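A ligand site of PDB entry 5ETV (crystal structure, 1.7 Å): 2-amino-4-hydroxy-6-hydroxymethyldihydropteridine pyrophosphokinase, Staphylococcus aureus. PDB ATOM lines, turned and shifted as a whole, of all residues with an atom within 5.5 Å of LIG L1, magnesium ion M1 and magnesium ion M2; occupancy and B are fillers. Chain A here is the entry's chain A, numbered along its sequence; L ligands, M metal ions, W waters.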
ATOM      1  N   LEU A  74     -15.739  21.990  -8.165  1.00  0.00           N
ATOM      2  CA  LEU A  74     -16.912  21.147  -8.324  1.00  0.00           C
ATOM      3  C   LEU A  74     -18.037  21.568  -7.376  1.00  0.00           C
ATOM      4  O   LEU A  74     -19.188  21.679  -7.804  1.00  0.00           O
ATOM      5  CB  LEU A  74     -16.614  19.659  -8.109  1.00  0.00           C
ATOM      6  CG  LEU A  74     -17.872  18.740  -8.295  1.00  0.00           C
ATOM      7  CD1 LEU A  74     -18.359  18.741  -9.737  1.00  0.00           C
ATOM      8  CD2 LEU A  74     -17.532  17.325  -7.805  1.00  0.00           C
ATOM      9  N   LEU A  78     -21.831  22.815  -8.536  1.00  0.00           N
ATOM     10  CA  LEU A  78     -23.053  22.216  -7.987  1.00  0.00           C
ATOM     11  C   LEU A  78     -23.900  23.223  -7.235  1.00  0.00           C
ATOM     12  O   LEU A  78     -25.141  23.208  -7.351  1.00  0.00           O
ATOM     13  CB  LEU A  78     -22.708  21.012  -7.106  1.00  0.00           C
ATOM     14  CG  LEU A  78     -22.008  19.882  -7.832  1.00  0.00           C
ATOM     15  CD1 LEU A  78     -21.745  18.722  -6.889  1.00  0.00           C
ATOM     16  CD2 LEU A  78     -22.726  19.429  -9.088  1.00  0.00           C
ATOM     17  N   GLU A  81     -25.869  25.297  -9.709  1.00  0.00           N
ATOM     18  CA  GLU A  81     -27.104  24.576 -10.126  1.00  0.00           C
ATOM     19  C   GLU A  81     -28.208  24.696  -9.095  1.00  0.00           C
ATOM     20  O   GLU A  81     -29.394  24.943  -9.440  1.00  0.00           O
ATOM     21  CB  GLU A  81     -26.778  23.105 -10.398  1.00  0.00           C
ATOM     22  CG  GLU A  81     -25.785  22.844 -11.483  1.00  0.00           C
ATOM     23  CD  GLU A  81     -25.433  21.393 -11.636  1.00  0.00           C
ATOM     24  OE1 GLU A  81     -25.964  20.565 -10.831  1.00  0.00           O
ATOM     25  OE2 GLU A  81     -24.669  21.071 -12.558  1.00  0.00           O
ATOM     26  N   ARG A  86     -32.173  23.805  -9.875  1.00  0.00           N
ATOM     27  CA  ARG A  86     -32.136  22.484 -10.409  1.00  0.00           C
ATOM     28  C   ARG A  86     -32.679  21.508  -9.364  1.00  0.00           C
ATOM     29  O   ARG A  86     -32.059  21.284  -8.330  1.00  0.00           O
ATOM     30  CB  ARG A  86     -30.739  22.080 -10.858  1.00  0.00           C
ATOM     31  CG  ARG A  86     -30.765  20.739 -11.551  1.00  0.00           C
ATOM     32  CD  ARG A  86     -29.388  20.214 -11.882  1.00  0.00           C
ATOM     33  NE  ARG A  86     -29.498  18.910 -12.533  1.00  0.00           N
ATOM     34  CZ  ARG A  86     -28.490  18.243 -13.070  1.00  0.00           C
ATOM     35  NH1 ARG A  86     -27.257  18.718 -12.993  1.00  0.00           N
ATOM     36  NH2 ARG A  86     -28.712  17.052 -13.623  1.00  0.00           N
ATOM     37  N   LYS A  89     -32.653  15.544 -10.621  1.00  0.00           N
ATOM     38  CA  LYS A  89     -31.297  15.005 -10.510  1.00  0.00           C
ATOM     39  C   LYS A  89     -31.005  13.781 -11.395  1.00  0.00           C
ATOM     40  O   LYS A  89     -29.886  13.255 -11.348  1.00  0.00           O
ATOM     41  CB  LYS A  89     -31.022  14.702  -9.030  1.00  0.00           C
ATOM     42  CG  LYS A  89     -31.015  15.967  -8.163  1.00  0.00           C
ATOM     43  CD  LYS A  89     -29.899  16.964  -8.529  1.00  0.00           C
ATOM     44  CE  LYS A  89     -30.176  18.346  -7.971  1.00  0.00           C
ATOM     45  NZ  LYS A  89     -30.544  18.291  -6.517  1.00  0.00           N
ATOM     46  N   GLU A  90     -31.979  13.337 -12.209  1.00  0.00           N
ATOM     47  CA  GLU A  90     -31.777  12.206 -13.153  1.00  0.00           C
ATOM     48  C   GLU A  90     -30.762  12.664 -14.168  1.00  0.00           C
ATOM     49  O   GLU A  90     -30.974  13.659 -14.893  1.00  0.00           O
ATOM     50  CB  GLU A  90     -33.071  11.829 -13.915  1.00  0.00           C
ATOM     51  CG  GLU A  90     -34.203  11.314 -13.075  1.00  0.00           C
ATOM     52  CD  GLU A  90     -34.900  12.374 -12.247  1.00  0.00           C
ATOM     53  OE1 GLU A  90     -34.950  13.559 -12.669  1.00  0.00           O
ATOM     54  OE2 GLU A  90     -35.413  12.012 -11.160  1.00  0.00           O
ATOM     55  N   ARG A  91     -29.624  11.967 -14.242  1.00  0.00           N
ATOM     56  CA  ARG A  91     -28.554  12.410 -15.117  1.00  0.00           C
ATOM     57  C   ARG A  91     -29.010  12.430 -16.569  1.00  0.00           C
ATOM     58  O   ARG A  91     -28.544  13.231 -17.362  1.00  0.00           O
ATOM     59  CB  ARG A  91     -27.307  11.506 -14.954  1.00  0.00           C
ATOM     60  CG  ARG A  91     -26.767  11.550 -13.528  1.00  0.00           C
ATOM     61  CD  ARG A  91     -25.712  10.493 -13.273  1.00  0.00           C
ATOM     62  NE  ARG A  91     -24.787  10.548 -14.371  1.00  0.00           N
ATOM     63  CZ  ARG A  91     -23.471  10.783 -14.271  1.00  0.00           C
ATOM     64  NH1 ARG A  91     -22.883  10.895 -13.061  1.00  0.00           N
ATOM     65  NH2 ARG A  91     -22.761  10.832 -15.400  1.00  0.00           N
ATOM     66  N   TRP A  92     -29.935  11.547 -16.913  1.00  0.00           N
ATOM     67  CA  TRP A  92     -30.411  11.459 -18.299  1.00  0.00           C
ATOM     68  C   TRP A  92     -31.481  12.508 -18.656  1.00  0.00           C
ATOM     69  O   TRP A  92     -31.783  12.676 -19.836  1.00  0.00           O
ATOM     70  CB  TRP A  92     -30.991  10.047 -18.567  1.00  0.00           C
ATOM     71  CG  TRP A  92     -32.027   9.572 -17.578  1.00  0.00           C
ATOM     72  CD1 TRP A  92     -31.799   8.769 -16.499  1.00  0.00           C
ATOM     73  CD2 TRP A  92     -33.433   9.858 -17.578  1.00  0.00           C
ATOM     74  NE1 TRP A  92     -32.943   8.535 -15.831  1.00  0.00           N
ATOM     75  CE2 TRP A  92     -33.975   9.192 -16.454  1.00  0.00           C
ATOM     76  CE3 TRP A  92     -34.276  10.621 -18.401  1.00  0.00           C
ATOM     77  CZ2 TRP A  92     -35.344   9.225 -16.151  1.00  0.00           C
ATOM     78  CZ3 TRP A  92     -35.659  10.644 -18.082  1.00  0.00           C
ATOM     79  CH2 TRP A  92     -36.139   9.990 -16.969  1.00  0.00           C
ATOM     80  N   ARG A  95     -32.946  19.655 -17.077  1.00  0.00           N
ATOM     81  CA  ARG A  95     -32.436  20.446 -15.955  1.00  0.00           C
ATOM     82  C   ARG A  95     -32.455  21.933 -16.300  1.00  0.00           C
ATOM     83  O   ARG A  95     -32.228  22.305 -17.455  1.00  0.00           O
ATOM     84  CB  ARG A  95     -31.017  20.005 -15.532  1.00  0.00           C
ATOM     85  CG  ARG A  95     -29.871  20.301 -16.494  1.00  0.00           C
ATOM     86  CD  ARG A  95     -29.844  19.528 -17.815  1.00  0.00           C
ATOM     87  NE  ARG A  95     -29.903  18.087 -17.547  1.00  0.00           N
ATOM     88  CZ  ARG A  95     -28.857  17.295 -17.296  1.00  0.00           C
ATOM     89  NH1 ARG A  95     -27.647  17.803 -17.262  1.00  0.00           N
ATOM     90  NH2 ARG A  95     -29.020  16.028 -16.972  1.00  0.00           N
ATOM     91  N   ASP A  98     -26.999  22.933 -15.848  1.00  0.00           N
ATOM     92  CA  ASP A  98     -25.918  21.941 -15.652  1.00  0.00           C
ATOM     93  C   ASP A  98     -24.596  22.706 -15.793  1.00  0.00           C
ATOM     94  O   ASP A  98     -24.395  23.412 -16.795  1.00  0.00           O
ATOM     95  CB  ASP A  98     -26.039  20.921 -16.774  1.00  0.00           C
ATOM     96  CG  ASP A  98     -25.050  19.781 -16.658  1.00  0.00           C
ATOM     97  OD1 ASP A  98     -24.716  19.398 -15.531  1.00  0.00           O
ATOM     98  OD2 ASP A  98     -24.618  19.266 -17.738  1.00  0.00           O
ATOM     99  N   VAL A  99     -23.710  22.551 -14.828  1.00  0.00           N
ATOM    100  CA  VAL A  99     -22.377  23.141 -14.898  1.00  0.00           C
ATOM    101  C   VAL A  99     -21.375  21.983 -14.777  1.00  0.00           C
ATOM    102  O   VAL A  99     -21.238  21.364 -13.699  1.00  0.00           O
ATOM    103  CB  VAL A  99     -22.171  24.212 -13.793  1.00  0.00           C
ATOM    104  CG1 VAL A  99     -20.829  24.905 -13.976  1.00  0.00           C
ATOM    105  CG2 VAL A  99     -23.332  25.204 -13.781  1.00  0.00           C
ATOM    106  N   ASP A 100     -20.648  21.729 -15.873  1.00  0.00           N
ATOM    107  CA  ASP A 100     -19.692  20.633 -15.967  1.00  0.00           C
ATOM    108  C   ASP A 100     -18.271  21.179 -16.038  1.00  0.00           C
ATOM    109  O   ASP A 100     -18.038  22.150 -16.762  1.00  0.00           O
ATOM    110  CB  ASP A 100     -19.973  19.759 -17.185  1.00  0.00           C
ATOM    111  CG  ASP A 100     -21.303  19.017 -17.060  1.00  0.00           C
ATOM    112  OD1 ASP A 100     -21.816  18.904 -15.941  1.00  0.00           O
ATOM    113  OD2 ASP A 100     -21.768  18.531 -18.088  1.00  0.00           O
ATOM    114  N   ILE A 101     -17.365  20.557 -15.315  1.00  0.00           N
ATOM    115  CA  ILE A 101     -15.954  20.907 -15.424  1.00  0.00           C
ATOM    116  C   ILE A 101     -15.382  20.171 -16.616  1.00  0.00           C
ATOM    117  O   ILE A 101     -15.322  18.944 -16.624  1.00  0.00           O
ATOM    118  CB  ILE A 101     -15.146  20.593 -14.174  1.00  0.00           C
ATOM    119  CG1 ILE A 101     -15.660  21.354 -12.947  1.00  0.00           C
ATOM    120  CG2 ILE A 101     -13.670  20.960 -14.390  1.00  0.00           C
ATOM    121  CD1 ILE A 101     -15.085  20.934 -11.600  1.00  0.00           C
ATOM    122  N   LEU A 102     -14.927  20.892 -17.633  1.00  0.00           N
ATOM    123  CA  LEU A 102     -14.379  20.279 -18.811  1.00  0.00           C
ATOM    124  C   LEU A 102     -12.877  20.061 -18.683  1.00  0.00           C
ATOM    125  O   LEU A 102     -12.392  18.993 -19.002  1.00  0.00           O
ATOM    126  CB  LEU A 102     -14.679  21.138 -20.043  1.00  0.00           C
ATOM    127  CG  LEU A 102     -16.189  21.419 -20.261  1.00  0.00           C
ATOM    128  CD1 LEU A 102     -16.372  22.337 -21.468  1.00  0.00           C
ATOM    129  CD2 LEU A 102     -16.946  20.142 -20.472  1.00  0.00           C
ATOM    130  N   LYS A 113     -16.419   9.828  -8.651  1.00  0.00           N
ATOM    131  CA  LYS A 113     -17.406  10.866  -8.963  1.00  0.00           C
ATOM    132  C   LYS A 113     -16.861  12.274  -9.383  1.00  0.00           C
ATOM    133  O   LYS A 113     -17.527  13.321  -9.246  1.00  0.00           O
ATOM    134  CB  LYS A 113     -18.345  11.016  -7.776  1.00  0.00           C
ATOM    135  CG  LYS A 113     -18.862   9.679  -7.203  1.00  0.00           C
ATOM    136  CD  LYS A 113     -19.912   9.875  -6.123  1.00  0.00           C
ATOM    137  CE  LYS A 113     -20.408   8.525  -5.590  1.00  0.00           C
ATOM    138  NZ  LYS A 113     -21.784   8.643  -5.025  1.00  0.00           N
ATOM    139  N   LEU A 114     -15.624  12.317  -9.870  1.00  0.00           N
ATOM    140  CA  LEU A 114     -15.125  13.539 -10.495  1.00  0.00           C
ATOM    141  C   LEU A 114     -14.054  13.109 -11.477  1.00  0.00           C
ATOM    142  O   LEU A 114     -13.021  12.583 -11.050  1.00  0.00           O
ATOM    143  CB  LEU A 114     -14.550  14.522  -9.482  1.00  0.00           C
ATOM    144  CG  LEU A 114     -13.900  15.787 -10.084  1.00  0.00           C
ATOM    145  CD1 LEU A 114     -14.889  16.517 -11.005  1.00  0.00           C
ATOM    146  CD2 LEU A 114     -13.394  16.737  -9.048  1.00  0.00           C
ATOM    147  N   SER A 115     -14.321  13.278 -12.776  1.00  0.00           N
ATOM    148  CA  SER A 115     -13.371  12.985 -13.826  1.00  0.00           C
ATOM    149  C   SER A 115     -13.134  14.274 -14.599  1.00  0.00           C
ATOM    150  O   SER A 115     -14.070  14.897 -15.109  1.00  0.00           O
ATOM    151  CB  SER A 115     -13.752  11.860 -14.819  1.00  0.00           C
ATOM    152  OG  SER A 115     -13.608  10.524 -14.287  1.00  0.00           O
ATOM    153  N   VAL A 116     -11.874  14.654 -14.738  1.00  0.00           N
ATOM    154  CA  VAL A 116     -11.488  15.863 -15.472  1.00  0.00           C
ATOM    155  C   VAL A 116     -10.176  15.493 -16.155  1.00  0.00           C
ATOM    156  O   VAL A 116      -9.311  14.982 -15.497  1.00  0.00           O
ATOM    157  CB  VAL A 116     -11.204  17.082 -14.557  1.00  0.00           C
ATOM    158  CG1 VAL A 116     -10.766  18.283 -15.374  1.00  0.00           C
ATOM    159  CG2 VAL A 116     -12.420  17.412 -13.730  1.00  0.00           C
ATOM    160  N   PRO A 117      -9.993  15.755 -17.437  1.00  0.00           N
ATOM    161  CA  PRO A 117     -10.983  16.318 -18.345  1.00  0.00           C
ATOM    162  C   PRO A 117     -12.281  15.563 -18.339  1.00  0.00           C
ATOM    163  O   PRO A 117     -12.303  14.339 -18.062  1.00  0.00           O
ATOM    164  CB  PRO A 117     -10.285  16.206 -19.711  1.00  0.00           C
ATOM    165  CG  PRO A 117      -8.834  16.182 -19.438  1.00  0.00           C
ATOM    166  CD  PRO A 117      -8.736  15.436 -18.119  1.00  0.00           C
ATOM    167  N   HIS A 118     -13.380  16.281 -18.596  1.00  0.00           N
ATOM    168  CA  HIS A 118     -14.670  15.588 -18.632  1.00  0.00           C
ATOM    169  C   HIS A 118     -14.583  14.412 -19.601  1.00  0.00           C
ATOM    170  O   HIS A 118     -14.175  14.587 -20.734  1.00  0.00           O
ATOM    171  CB  HIS A 118     -15.775  16.513 -19.035  1.00  0.00           C
ATOM    172  CG  HIS A 118     -17.122  15.964 -18.736  1.00  0.00           C
ATOM    173  ND1 HIS A 118     -17.678  14.965 -19.492  1.00  0.00           N
ATOM    174  CD2 HIS A 118     -18.021  16.257 -17.758  1.00  0.00           C
ATOM    175  CE1 HIS A 118     -18.866  14.655 -18.993  1.00  0.00           C
ATOM    176  NE2 HIS A 118     -19.098  15.403 -17.941  1.00  0.00           N
ATOM    177  N   PRO A 119     -14.916  13.193 -19.140  1.00  0.00           N
ATOM    178  CA  PRO A 119     -14.538  12.024 -19.957  1.00  0.00           C
ATOM    179  C   PRO A 119     -15.388  11.801 -21.208  1.00  0.00           C
ATOM    180  O   PRO A 119     -15.018  10.997 -22.057  1.00  0.00           O
ATOM    181  CB  PRO A 119     -14.643  10.849 -18.970  1.00  0.00           C
ATOM    182  CG  PRO A 119     -15.519  11.305 -17.938  1.00  0.00           C
ATOM    183  CD  PRO A 119     -15.391  12.817 -17.813  1.00  0.00           C
ATOM    184  N   ARG A 120     -16.483  12.545 -21.327  1.00  0.00           N
ATOM    185  CA  ARG A 120     -17.384  12.434 -22.480  1.00  0.00           C
ATOM    186  C   ARG A 120     -17.290  13.590 -23.464  1.00  0.00           C
ATOM    187  O   ARG A 120     -17.947  13.517 -24.510  1.00  0.00           O
ATOM    188  CB  ARG A 120     -18.828  12.224 -21.971  1.00  0.00           C
ATOM    189  CG  ARG A 120     -18.885  10.789 -21.342  1.00  0.00           C
ATOM    190  CD  ARG A 120     -20.125  10.598 -20.543  1.00  0.00           C
ATOM    191  NE  ARG A 120     -20.035  11.204 -19.228  1.00  0.00           N
ATOM    192  CZ  ARG A 120     -19.344  10.684 -18.213  1.00  0.00           C
ATOM    193  NH1 ARG A 120     -18.651   9.527 -18.366  1.00  0.00           N
ATOM    194  NH2 ARG A 120     -19.356  11.324 -17.031  1.00  0.00           N
ATOM    195  N   ARG A 124     -18.896  14.955 -27.958  1.00  0.00           N
ATOM    196  CA  ARG A 124     -20.069  15.815 -27.821  1.00  0.00           C
ATOM    197  C   ARG A 124     -19.867  17.128 -28.581  1.00  0.00           C
ATOM    198  O   ARG A 124     -19.157  18.004 -28.119  1.00  0.00           O
ATOM    199  CB  ARG A 124     -20.318  16.125 -26.348  1.00  0.00           C
ATOM    200  CG  ARG A 124     -20.817  14.915 -25.585  1.00  0.00           C
ATOM    201  CD  ARG A 124     -20.823  15.288 -24.110  1.00  0.00           C
ATOM    202  NE  ARG A 124     -21.450  14.213 -23.327  1.00  0.00           N
ATOM    203  CZ  ARG A 124     -21.781  14.317 -22.058  1.00  0.00           C
ATOM    204  NH1 ARG A 124     -21.522  15.410 -21.353  1.00  0.00           N
ATOM    205  NH2 ARG A 124     -22.335  13.298 -21.436  1.00  0.00           N
HETATM  206  P1  LIG L   1     -22.377  14.659 -17.862  1.00  0.00           P
HETATM  207  O1  LIG L   1     -22.548  15.840 -18.784  1.00  0.00           O
HETATM  208  O2  LIG L   1     -21.529  14.902 -16.652  1.00  0.00           O
HETATM  209  O3  LIG L   1     -22.089  13.390 -18.620  1.00  0.00           O
HETATM  210  P2  LIG L   1     -24.669  15.343 -16.331  1.00  0.00           P
HETATM  211  O4  LIG L   1     -23.996  16.699 -16.342  1.00  0.00           O
HETATM  212  O5  LIG L   1     -26.189  15.312 -16.774  1.00  0.00           O
HETATM  213  O6  LIG L   1     -23.862  14.338 -17.280  1.00  0.00           O
HETATM  214  P3  LIG L   1     -25.019  15.635 -13.338  1.00  0.00           P
HETATM  215  O7  LIG L   1     -24.825  17.150 -13.650  1.00  0.00           O
HETATM  216  O8  LIG L   1     -26.428  15.279 -13.008  1.00  0.00           O
HETATM  217  C1  LIG L   1     -24.459  14.603 -14.690  1.00  0.00           C
HETATM  218  O9  LIG L   1     -23.975  15.480 -12.111  1.00  0.00           O
HETATM  219  C2  LIG L   1     -23.774  14.282 -11.434  1.00  0.00           C
HETATM  220  C3  LIG L   1     -22.373  14.224 -10.848  1.00  0.00           C
HETATM  221  O10 LIG L   1     -21.418  14.125 -11.922  1.00  0.00           O
HETATM  222  C4  LIG L   1     -21.803  15.347  -9.996  1.00  0.00           C
HETATM  223  O11 LIG L   1     -22.325  15.391  -8.674  1.00  0.00           O
HETATM  224  C5  LIG L   1     -20.343  14.960  -9.988  1.00  0.00           C
HETATM  225  O12 LIG L   1     -20.023  14.196  -8.812  1.00  0.00           O
HETATM  226  C6  LIG L   1     -20.191  14.086 -11.231  1.00  0.00           C
HETATM  227  N1  LIG L   1     -19.084  14.512 -12.098  1.00  0.00           N
HETATM  228  C7  LIG L   1     -18.073  13.718 -12.494  1.00  0.00           C
HETATM  229  N2  LIG L   1     -17.184  14.429 -13.250  1.00  0.00           N
HETATM  230  C8  LIG L   1     -17.687  15.688 -13.372  1.00  0.00           C
HETATM  231  C9  LIG L   1     -17.252  16.916 -14.069  1.00  0.00           C
HETATM  232  N3  LIG L   1     -16.081  16.844 -14.761  1.00  0.00           N
HETATM  233  N4  LIG L   1     -18.039  18.015 -13.940  1.00  0.00           N
HETATM  234  C10 LIG L   1     -19.199  18.005 -13.224  1.00  0.00           C
HETATM  235  N5  LIG L   1     -19.654  16.905 -12.566  1.00  0.00           N
HETATM  236  C11 LIG L   1     -18.937  15.746 -12.610  1.00  0.00           C
HETATM  237  C1  LG2 L   2     -25.964  11.005 -21.979  1.00  0.00           C
HETATM  238  C2  LG2 L   2     -25.086  11.547 -24.130  1.00  0.00           C
HETATM  239  C3  LG2 L   2     -26.155   9.708 -22.411  1.00  0.00           C
HETATM  240  C4  LG2 L   2     -25.289  10.254 -24.557  1.00  0.00           C
HETATM  241  C5  LG2 L   2     -25.418  11.936 -22.836  1.00  0.00           C
HETATM  242  C6  LG2 L   2     -26.835  17.493 -22.627  1.00  0.00           C
HETATM  243  C7  LG2 L   2     -25.820   9.327 -23.683  1.00  0.00           C
HETATM  244  C8  LG2 L   2     -27.455  16.742 -23.591  1.00  0.00           C
HETATM  245  C9  LG2 L   2     -26.434  18.846 -22.956  1.00  0.00           C
HETATM  246  C10 LG2 L   2     -27.408  18.304 -25.145  1.00  0.00           C
HETATM  247  C11 LG2 L   2     -27.211  15.592 -21.770  1.00  0.00           C
HETATM  248  C12 LG2 L   2     -25.218  13.340 -22.392  1.00  0.00           C
HETATM  249  C13 LG2 L   2     -25.504  13.817 -20.973  1.00  0.00           C
HETATM  250  N1  LG2 L   2     -27.773  17.094 -24.842  1.00  0.00           N
HETATM  251  N2  LG2 L   2     -27.714  15.516 -23.030  1.00  0.00           N
HETATM  252  N3  LG2 L   2     -26.757  19.146 -24.250  1.00  0.00           N
HETATM  253  N4  LG2 L   2     -26.681  16.748 -21.476  1.00  0.00           N
HETATM  254  N5  LG2 L   2     -27.630  18.858 -26.387  1.00  0.00           N
HETATM  255  O1  LG2 L   2     -24.815  14.141 -23.227  1.00  0.00           O
HETATM  256  O2  LG2 L   2     -25.886  19.634 -22.219  1.00  0.00           O
HETATM  257  S1  LG2 L   2     -27.261  14.241 -20.652  1.00  0.00           S
HETATM  258 BR1  LG2 L   2     -26.143   7.514 -24.168  1.00  0.00          BR
HETATM  259 MG    MG M   1     -23.595  17.576 -18.404  1.00  0.00          MG
HETATM  260 MG    MG M   2     -23.407  18.009 -14.872  1.00  0.00          MG
HETATM  261  O   HOH W   1     -22.862  19.146 -13.268  1.00  0.00           O
HETATM  262  O   HOH W   2     -23.576  18.365 -20.304  1.00  0.00           O
HETATM  263  O   HOH W   3     -20.743  15.385  -5.973  1.00  0.00           O
HETATM  264  O   HOH W   4     -23.494  11.019 -17.924  1.00  0.00           O
HETATM  265  O   HOH W   5     -24.857  16.451  -8.600  1.00  0.00           O
HETATM  266  O   HOH W   6     -26.098  12.271 -18.229  1.00  0.00           O
HETATM  267  O   HOH W   7     -25.420  16.722 -19.087  1.00  0.00           O
HETATM  268  O   HOH W   8     -21.923  16.473 -14.452  1.00  0.00           O
HETATM  269  O   HOH W   9     -24.863  18.087 -10.821  1.00  0.00           O
HETATM  270  O   HOH W  10     -27.582  14.375 -10.863  1.00  0.00           O
HETATM  271  O   HOH W  11     -20.990  12.870 -14.809  1.00  0.00           O
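The backbone carbonyl oxygen (O) of Lys 113 sits at hydrogen-bond distance from an oxygen (O12) of LIG L1 (2.7 Å).
NE2 of His 118 lies within hydrogen-bond range of O2 of LIG L1 (2.8 Å).
NH2 of Arg 124 is in salt-bridge range of O3 of LIG L1 (2.8 Å).
N2 of LIG L1 sits at hydrogen-bond distance from N of Ser 115.
A nitrogen (N3) of LIG L1 lies within hydrogen-bond range of the backbone carbonyl oxygen of Ser 115 (2.8 Å).
N of Ile 101 is in hydrogen-bond range of N4 of LIG L1 (3.0 Å).
O of Ile 101 lies within hydrogen-bond range of N3 of LIG L1 (2.9 Å).
NH2 of Arg 95 lies within salt-bridge range of O5 of LIG L1, at 2.9 Å.
O8 of LIG L1 lies within salt-bridge range of NH2 of Arg 86 (3.0 Å).
O3 of LIG L1 lies within salt-bridge range of NE of Arg 120, at 3.1 Å.
NH2 of Arg 124 sits close to O1 of LG2 L2 (3.2 Å).
OD2 of Asp 98 sits close to NH1 of Arg 95, at 3.4 Å.
The guanidinium group (NH1) of Arg 86 sits close to the side-chain carboxylate (OD1) of Asp 98 (3.7 Å).
N of Arg 120 sits close to ND1 of His 118.
N of His 118 is in hydrogen-bond range of O of Leu 102 (2.9 Å).
NH2 of Arg 95 lies within hydrogen-bond range of O of Arg 91.
The guanidinium group of Arg 86 lies within salt-bridge range of the side-chain carboxylate of Glu 81, at 3.1 Å.
OE2 of Glu 81 is in hydrogen-bond range of N of Val 99 (2.9 Å).
O of Arg 91 lies close to O5 of LIG L1, at 3.2 Å.
Residues that only touch LIG L1: Leu 74 (3.6 Å), Leu 78 (3.8 Å), Val 99 (3.96 Å), Leu 114 (3.6 Å) and Val 116 (3.8 Å).
Hydrophobic or aromatic side chains that line LIG L1: Leu 74, Leu 78, Ile 101, Leu 114, Val 116 and His 118.
Two residues have an atom within 4 Å of magnesium ion M1: Asp 98 and Asp 100.
Of the 23 residues printed, 2 come within 4 Å of magnesium ion M2.
The nearest printed residue that does not touch magnesium ion M2 is Glu 81 (4.04 Å).
Magnesium ion M1 is bound by water W2 (2.1 Å), O1 of LIG L1 (2.1 Å), OD2 of Asp 98 (2.1 Å), OD2 of Asp 100 (2.1 Å), water W7 (2.1 Å) and O4 of LIG L1 (2.3 Å).
Magnesium ion M1 has six donor atoms within binding distance.
Magnesium ion M2 is bound by the side-chain carboxylate of Asp 98 (2.0 Å), water W1 (2.0 Å), an oxygen (O4) of LIG L1 (2.1 Å), an oxygen (O7) of LIG L1 (2.1 Å), the side-chain carboxylate of Asp 100 (2.1 Å) and water W8 (2.2 Å).
Water W7 lies within hydrogen-bond range of a nitrogen (N4) of LG2 L2, an oxygen (O5) of LIG L1 and the guanidinium group (NH1) of Arg 95.
Water W1 bridges the side-chain carboxylate (OE2) of Glu 81 (2.7 Å) and the backbone carbonyl oxygen (O) of Val 99 (2.8 Å).
Water W10 bridges O8 of LIG L1 (2.6 Å) and O of Lys 89 (2.6 Å).
Water W11 lies within hydrogen-bond range of the guanidinium group (NH2) of Arg 91, an oxygen (O2) of LIG L1 and the guanidinium group (NH2) of Arg 120.
Water W4 bridges NH2 of Arg 91 and O3 of LIG L1.
Water W9 lies within hydrogen-bond range of OE1 of Glu 81 (2.7 Å), O9 of LIG L1 (3.0 Å) and NH1 of Arg 86 (3.3 Å).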
